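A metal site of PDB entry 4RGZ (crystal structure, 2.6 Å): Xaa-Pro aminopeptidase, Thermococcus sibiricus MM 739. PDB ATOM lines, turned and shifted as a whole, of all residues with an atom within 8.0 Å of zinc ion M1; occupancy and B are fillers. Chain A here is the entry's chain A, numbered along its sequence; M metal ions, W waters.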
ATOM      1  N   PHE A 195     -27.882   1.054  14.586  1.00  0.00           N
ATOM      2  CA  PHE A 195     -28.685   1.131  13.351  1.00  0.00           C
ATOM      3  C   PHE A 195     -27.785   0.838  12.147  1.00  0.00           C
ATOM      4  O   PHE A 195     -26.567   0.909  12.250  1.00  0.00           O
ATOM      5  CB  PHE A 195     -29.354   2.493  13.191  1.00  0.00           C
ATOM      6  CG  PHE A 195     -28.405   3.650  13.217  1.00  0.00           C
ATOM      7  CD1 PHE A 195     -27.956   4.182  14.434  1.00  0.00           C
ATOM      8  CD2 PHE A 195     -27.957   4.219  12.020  1.00  0.00           C
ATOM      9  CE1 PHE A 195     -27.060   5.224  14.480  1.00  0.00           C
ATOM     10  CE2 PHE A 195     -27.066   5.313  12.051  1.00  0.00           C
ATOM     11  CZ  PHE A 195     -26.610   5.790  13.292  1.00  0.00           C
ATOM     12  N   ILE A 198     -25.256   4.600   7.290  1.00  0.00           N
ATOM     13  CA  ILE A 198     -25.622   5.379   6.125  1.00  0.00           C
ATOM     14  C   ILE A 198     -24.395   6.016   5.477  1.00  0.00           C
ATOM     15  O   ILE A 198     -23.623   6.757   6.099  1.00  0.00           O
ATOM     16  CB  ILE A 198     -26.553   6.534   6.513  1.00  0.00           C
ATOM     17  CG1 ILE A 198     -27.837   6.046   7.193  1.00  0.00           C
ATOM     18  CG2 ILE A 198     -26.879   7.385   5.306  1.00  0.00           C
ATOM     19  CD1 ILE A 198     -28.437   7.089   8.149  1.00  0.00           C
ATOM     20  N   PHE A 225     -20.998  10.117   6.101  1.00  0.00           N
ATOM     21  CA  PHE A 225     -21.157   8.797   6.730  1.00  0.00           C
ATOM     22  C   PHE A 225     -21.623   8.854   8.194  1.00  0.00           C
ATOM     23  O   PHE A 225     -21.112   9.645   9.002  1.00  0.00           O
ATOM     24  CB  PHE A 225     -19.973   7.862   6.466  1.00  0.00           C
ATOM     25  CG  PHE A 225     -18.644   8.451   6.808  1.00  0.00           C
ATOM     26  CD1 PHE A 225     -18.116   9.516   6.080  1.00  0.00           C
ATOM     27  CD2 PHE A 225     -17.875   7.892   7.849  1.00  0.00           C
ATOM     28  CE1 PHE A 225     -16.852  10.027   6.404  1.00  0.00           C
ATOM     29  CE2 PHE A 225     -16.621   8.403   8.186  1.00  0.00           C
ATOM     30  CZ  PHE A 225     -16.098   9.456   7.456  1.00  0.00           C
ATOM     31  N   ASP A 226     -22.630   8.054   8.499  1.00  0.00           N
ATOM     32  CA  ASP A 226     -23.455   8.233   9.688  1.00  0.00           C
ATOM     33  C   ASP A 226     -23.715   6.818  10.194  1.00  0.00           C
ATOM     34  O   ASP A 226     -24.214   5.969   9.450  1.00  0.00           O
ATOM     35  CB  ASP A 226     -24.749   8.962   9.283  1.00  0.00           C
ATOM     36  CG  ASP A 226     -25.660   9.337  10.452  1.00  0.00           C
ATOM     37  OD1 ASP A 226     -25.392   8.964  11.615  1.00  0.00           O
ATOM     38  OD2 ASP A 226     -26.677  10.059  10.197  1.00  0.00           O
ATOM     39  N   TYR A 227     -23.312   6.553  11.432  1.00  0.00           N
ATOM     40  CA  TYR A 227     -23.316   5.186  11.949  1.00  0.00           C
ATOM     41  C   TYR A 227     -23.314   5.232  13.445  1.00  0.00           C
ATOM     42  O   TYR A 227     -23.340   6.321  14.041  1.00  0.00           O
ATOM     43  CB  TYR A 227     -22.110   4.369  11.391  1.00  0.00           C
ATOM     44  CG  TYR A 227     -20.766   4.999  11.656  1.00  0.00           C
ATOM     45  CD1 TYR A 227     -20.373   6.180  11.014  1.00  0.00           C
ATOM     46  CD2 TYR A 227     -19.872   4.432  12.573  1.00  0.00           C
ATOM     47  CE1 TYR A 227     -19.139   6.761  11.282  1.00  0.00           C
ATOM     48  CE2 TYR A 227     -18.651   5.018  12.846  1.00  0.00           C
ATOM     49  CZ  TYR A 227     -18.275   6.165  12.209  1.00  0.00           C
ATOM     50  OH  TYR A 227     -17.032   6.732  12.491  1.00  0.00           O
ATOM     51  N   GLY A 228     -23.314   4.065  14.070  1.00  0.00           N
ATOM     52  CA  GLY A 228     -23.372   3.992  15.510  1.00  0.00           C
ATOM     53  C   GLY A 228     -23.214   2.598  16.060  1.00  0.00           C
ATOM     54  O   GLY A 228     -23.452   1.597  15.380  1.00  0.00           O
ATOM     55  N   SER A 236     -24.491   4.944  20.486  1.00  0.00           N
ATOM     56  CA  SER A 236     -23.831   6.111  19.974  1.00  0.00           C
ATOM     57  C   SER A 236     -24.262   6.298  18.543  1.00  0.00           C
ATOM     58  O   SER A 236     -24.964   5.420  17.954  1.00  0.00           O
ATOM     59  CB  SER A 236     -22.326   5.926  20.033  1.00  0.00           C
ATOM     60  OG  SER A 236     -21.890   4.937  19.139  1.00  0.00           O
ATOM     61  N   ASP A 237     -23.847   7.424  17.964  1.00  0.00           N
ATOM     62  CA  ASP A 237     -24.411   7.923  16.705  1.00  0.00           C
ATOM     63  C   ASP A 237     -23.535   9.097  16.256  1.00  0.00           C
ATOM     64  O   ASP A 237     -23.581  10.218  16.814  1.00  0.00           O
ATOM     65  CB  ASP A 237     -25.850   8.389  16.950  1.00  0.00           C
ATOM     66  CG  ASP A 237     -26.573   8.799  15.684  1.00  0.00           C
ATOM     67  OD1 ASP A 237     -26.037   8.607  14.559  1.00  0.00           O
ATOM     68  OD2 ASP A 237     -27.705   9.339  15.803  1.00  0.00           O
ATOM     69  N   VAL A 238     -22.733   8.863  15.218  1.00  0.00           N
ATOM     70  CA  VAL A 238     -21.867   9.890  14.744  1.00  0.00           C
ATOM     71  C   VAL A 238     -22.073  10.032  13.236  1.00  0.00           C
ATOM     72  O   VAL A 238     -22.457   9.053  12.549  1.00  0.00           O
ATOM     73  CB  VAL A 238     -20.428   9.527  15.133  1.00  0.00           C
ATOM     74  CG1 VAL A 238     -19.911   8.383  14.296  1.00  0.00           C
ATOM     75  CG2 VAL A 238     -19.516  10.732  15.042  1.00  0.00           C
ATOM     76  N   THR A 239     -21.871  11.249  12.746  1.00  0.00           N
ATOM     77  CA  THR A 239     -21.861  11.565  11.324  1.00  0.00           C
ATOM     78  C   THR A 239     -20.607  12.406  11.009  1.00  0.00           C
ATOM     79  O   THR A 239     -20.268  13.349  11.729  1.00  0.00           O
ATOM     80  CB  THR A 239     -23.117  12.396  10.910  1.00  0.00           C
ATOM     81  OG1 THR A 239     -24.327  11.690  11.204  1.00  0.00           O
ATOM     82  CG2 THR A 239     -23.113  12.689   9.427  1.00  0.00           C
ATOM     83  N   ARG A 240     -19.918  12.091   9.910  1.00  0.00           N
ATOM     84  CA  ARG A 240     -18.819  12.946   9.468  1.00  0.00           C
ATOM     85  C   ARG A 240     -18.850  13.113   7.942  1.00  0.00           C
ATOM     86  O   ARG A 240     -19.376  12.257   7.214  1.00  0.00           O
ATOM     87  CB  ARG A 240     -17.477  12.387   9.937  1.00  0.00           C
ATOM     88  CG  ARG A 240     -17.247  12.517  11.441  1.00  0.00           C
ATOM     89  CD  ARG A 240     -17.040  13.983  11.871  1.00  0.00           C
ATOM     90  NE  ARG A 240     -16.631  14.133  13.267  1.00  0.00           N
ATOM     91  CZ  ARG A 240     -17.449  14.175  14.322  1.00  0.00           C
ATOM     92  NH1 ARG A 240     -18.767  14.098  14.189  1.00  0.00           N
ATOM     93  NH2 ARG A 240     -16.935  14.298  15.539  1.00  0.00           N
ATOM     94  N   HIS A 301     -31.541  14.330  18.357  1.00  0.00           N
ATOM     95  CA  HIS A 301     -32.352  13.452  19.181  1.00  0.00           C
ATOM     96  C   HIS A 301     -31.553  12.881  20.329  1.00  0.00           C
ATOM     97  O   HIS A 301     -30.328  12.911  20.319  1.00  0.00           O
ATOM     98  CB  HIS A 301     -32.834  12.311  18.314  1.00  0.00           C
ATOM     99  CG  HIS A 301     -31.725  11.682  17.508  1.00  0.00           C
ATOM    100  ND1 HIS A 301     -30.958  10.673  17.975  1.00  0.00           N
ATOM    101  CD2 HIS A 301     -31.222  12.009  16.248  1.00  0.00           C
ATOM    102  CE1 HIS A 301     -30.039  10.341  17.058  1.00  0.00           C
ATOM    103  NE2 HIS A 301     -30.198  11.155  15.989  1.00  0.00           N
ATOM    104  N   LEU A 303     -30.091   9.830  23.010  1.00  0.00           N
ATOM    105  CA  LEU A 303     -29.555   8.485  22.951  1.00  0.00           C
ATOM    106  C   LEU A 303     -29.793   7.791  24.288  1.00  0.00           C
ATOM    107  O   LEU A 303     -29.742   8.413  25.340  1.00  0.00           O
ATOM    108  CB  LEU A 303     -28.058   8.526  22.630  1.00  0.00           C
ATOM    109  CG  LEU A 303     -27.746   9.287  21.349  1.00  0.00           C
ATOM    110  CD1 LEU A 303     -26.287   9.745  21.296  1.00  0.00           C
ATOM    111  CD2 LEU A 303     -28.182   8.515  20.102  1.00  0.00           C
ATOM    112  N   VAL A 307     -31.771   4.509  19.867  1.00  0.00           N
ATOM    113  CA  VAL A 307     -31.114   5.582  19.117  1.00  0.00           C
ATOM    114  C   VAL A 307     -31.931   6.869  19.006  1.00  0.00           C
ATOM    115  O   VAL A 307     -31.365   7.946  18.761  1.00  0.00           O
ATOM    116  CB  VAL A 307     -30.783   5.209  17.673  1.00  0.00           C
ATOM    117  CG1 VAL A 307     -29.358   5.656  17.376  1.00  0.00           C
ATOM    118  CG2 VAL A 307     -30.969   3.728  17.374  1.00  0.00           C
ATOM    119  N   HIS A 308     -33.249   6.782  19.132  1.00  0.00           N
ATOM    120  CA  HIS A 308     -34.039   7.995  19.239  1.00  0.00           C
ATOM    121  C   HIS A 308     -34.807   7.938  20.508  1.00  0.00           C
ATOM    122  O   HIS A 308     -35.624   7.033  20.759  1.00  0.00           O
ATOM    123  CB  HIS A 308     -34.980   8.158  18.048  1.00  0.00           C
ATOM    124  CG  HIS A 308     -34.287   8.474  16.733  1.00  0.00           C
ATOM    125  ND1 HIS A 308     -32.947   8.440  16.583  1.00  0.00           N
ATOM    126  CD2 HIS A 308     -34.811   8.849  15.499  1.00  0.00           C
ATOM    127  CE1 HIS A 308     -32.619   8.760  15.326  1.00  0.00           C
ATOM    128  NE2 HIS A 308     -33.770   9.019  14.660  1.00  0.00           N
ATOM    129  N   THR A 328     -27.745  14.064  20.439  1.00  0.00           N
ATOM    130  CA  THR A 328     -26.955  14.464  19.266  1.00  0.00           C
ATOM    131  C   THR A 328     -27.121  15.928  18.948  1.00  0.00           C
ATOM    132  O   THR A 328     -28.161  16.528  19.258  1.00  0.00           O
ATOM    133  CB  THR A 328     -27.378  13.688  18.015  1.00  0.00           C
ATOM    134  OG1 THR A 328     -28.751  13.981  17.715  1.00  0.00           O
ATOM    135  CG2 THR A 328     -27.188  12.173  18.233  1.00  0.00           C
ATOM    136  N   GLU A 330     -26.469  17.792  15.338  1.00  0.00           N
ATOM    137  CA  GLU A 330     -26.202  17.375  13.929  1.00  0.00           C
ATOM    138  C   GLU A 330     -26.906  18.255  12.868  1.00  0.00           C
ATOM    139  O   GLU A 330     -27.646  17.763  12.015  1.00  0.00           O
ATOM    140  CB  GLU A 330     -26.525  15.873  13.704  1.00  0.00           C
ATOM    141  CG  GLU A 330     -27.953  15.436  14.027  1.00  0.00           C
ATOM    142  CD  GLU A 330     -28.340  13.974  13.703  1.00  0.00           C
ATOM    143  OE1 GLU A 330     -27.671  13.245  12.930  1.00  0.00           O
ATOM    144  OE2 GLU A 330     -29.363  13.540  14.254  1.00  0.00           O
ATOM    145  N   ARG A 342     -23.424  17.049   6.941  1.00  0.00           N
ATOM    146  CA  ARG A 342     -23.900  16.920   8.313  1.00  0.00           C
ATOM    147  C   ARG A 342     -22.719  16.564   9.221  1.00  0.00           C
ATOM    148  O   ARG A 342     -21.850  15.769   8.839  1.00  0.00           O
ATOM    149  CB  ARG A 342     -25.008  15.870   8.421  1.00  0.00           C
ATOM    150  CG  ARG A 342     -25.616  15.723   9.835  1.00  0.00           C
ATOM    151  CD  ARG A 342     -26.343  14.402  10.075  1.00  0.00           C
ATOM    152  NE  ARG A 342     -27.129  14.156   8.892  1.00  0.00           N
ATOM    153  CZ  ARG A 342     -27.068  13.108   8.082  1.00  0.00           C
ATOM    154  NH1 ARG A 342     -26.329  12.039   8.341  1.00  0.00           N
ATOM    155  NH2 ARG A 342     -27.823  13.146   7.006  1.00  0.00           N
ATOM    156  N   ILE A 343     -22.673  17.159  10.407  1.00  0.00           N
ATOM    157  CA  ILE A 343     -21.629  16.878  11.410  1.00  0.00           C
ATOM    158  C   ILE A 343     -22.378  16.609  12.724  1.00  0.00           C
ATOM    159  O   ILE A 343     -23.133  17.449  13.220  1.00  0.00           O
ATOM    160  CB  ILE A 343     -20.627  18.052  11.579  1.00  0.00           C
ATOM    161  CG1 ILE A 343     -19.914  18.393  10.256  1.00  0.00           C
ATOM    162  CG2 ILE A 343     -19.601  17.759  12.671  1.00  0.00           C
ATOM    163  CD1 ILE A 343     -19.146  19.716  10.288  1.00  0.00           C
ATOM    164  N   GLU A 344     -22.182  15.412  13.264  1.00  0.00           N
ATOM    165  CA  GLU A 344     -22.928  14.937  14.411  1.00  0.00           C
ATOM    166  C   GLU A 344     -21.986  14.497  15.509  1.00  0.00           C
ATOM    167  O   GLU A 344     -20.988  13.775  15.301  1.00  0.00           O
ATOM    168  CB  GLU A 344     -23.771  13.746  13.986  1.00  0.00           C
ATOM    169  CG  GLU A 344     -24.809  13.292  15.013  1.00  0.00           C
ATOM    170  CD  GLU A 344     -25.504  12.005  14.603  1.00  0.00           C
ATOM    171  OE1 GLU A 344     -24.975  11.264  13.722  1.00  0.00           O
ATOM    172  OE2 GLU A 344     -26.593  11.730  15.158  1.00  0.00           O
ATOM    173  N   ASP A 345     -22.298  14.937  16.720  1.00  0.00           N
ATOM    174  CA  ASP A 345     -21.590  14.513  17.899  1.00  0.00           C
ATOM    175  C   ASP A 345     -22.610  14.022  18.919  1.00  0.00           C
ATOM    176  O   ASP A 345     -23.814  14.347  18.867  1.00  0.00           O
ATOM    177  CB  ASP A 345     -20.784  15.683  18.490  1.00  0.00           C
ATOM    178  CG  ASP A 345     -19.441  15.927  17.778  1.00  0.00           C
ATOM    179  OD1 ASP A 345     -18.695  14.968  17.484  1.00  0.00           O
ATOM    180  OD2 ASP A 345     -19.096  17.097  17.559  1.00  0.00           O
ATOM    181  N   ASP A 346     -22.108  13.233  19.870  1.00  0.00           N
ATOM    182  CA  ASP A 346     -22.907  12.815  20.995  1.00  0.00           C
ATOM    183  C   ASP A 346     -22.482  13.686  22.169  1.00  0.00           C
ATOM    184  O   ASP A 346     -21.296  13.794  22.446  1.00  0.00           O
ATOM    185  CB  ASP A 346     -22.684  11.327  21.214  1.00  0.00           C
ATOM    186  CG  ASP A 346     -23.219  10.528  20.061  1.00  0.00           C
ATOM    187  OD1 ASP A 346     -23.945  11.166  19.253  1.00  0.00           O
ATOM    188  OD2 ASP A 346     -22.944   9.307  19.919  1.00  0.00           O
HETATM  189 ZN    ZN M   1     -26.581   9.934  13.079  1.00  0.00          ZN
HETATM  190 ZN    ZN M   2     -32.993  12.674  13.220  1.00  0.00          ZN
HETATM  191  O   HOH W   1     -28.571  10.569  13.128  1.00  0.00           O
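OD2 of Asp 237 sits close to NE2 of His 301.
The backbone NH of Asp 237 sits at hydrogen-bond distance from the side-chain carboxylate of Asp 346.
OD2 of Asp 226 sits close to OG1 of Thr 239, at 3.0 Å.
The side-chain carboxylate (OD2) of Asp 226 is in salt-bridge range of the guanidinium group (NH1) of Arg 342 (2.7 Å).
The backbone carbonyl oxygen (O) of Asp 226 is in hydrogen-bond range of the backbone NH (N) of Ile 198, 2.8 Å away.
O of Thr 239 is in hydrogen-bond range of N of Glu 344, at 3.2 Å.
The backbone carbonyl oxygen of Glu 344 lies within hydrogen-bond range of the guanidinium group of Arg 240, 2.5 Å away.
The side-chain carboxylate of Glu 330 lies within hydrogen-bond range of a ring nitrogen (NE2) of His 301 (3.1 Å).
Residues that only touch zinc ion M1: Thr 239 (3.4 Å) and Glu 330 (3.5 Å).
Within 4 Å of zinc ion M1: Asp 226, Asp 237, Thr 239, Glu 330 and Glu 344.
Zinc ion M1 is bound by OD1 of Asp 237 (2.1 Å).
Water W1 binds zinc ion M1 (2.1 Å).
Zinc ion M1 is bound by the side-chain carboxylate (OD1) of Asp 226 (2.1 Å).
Zinc ion M1 is bound by OE1 of Glu 344, 2.2 Å away.
Slightly farther from zinc ion M1 lies OE2 of Glu 344 (2.7 Å).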
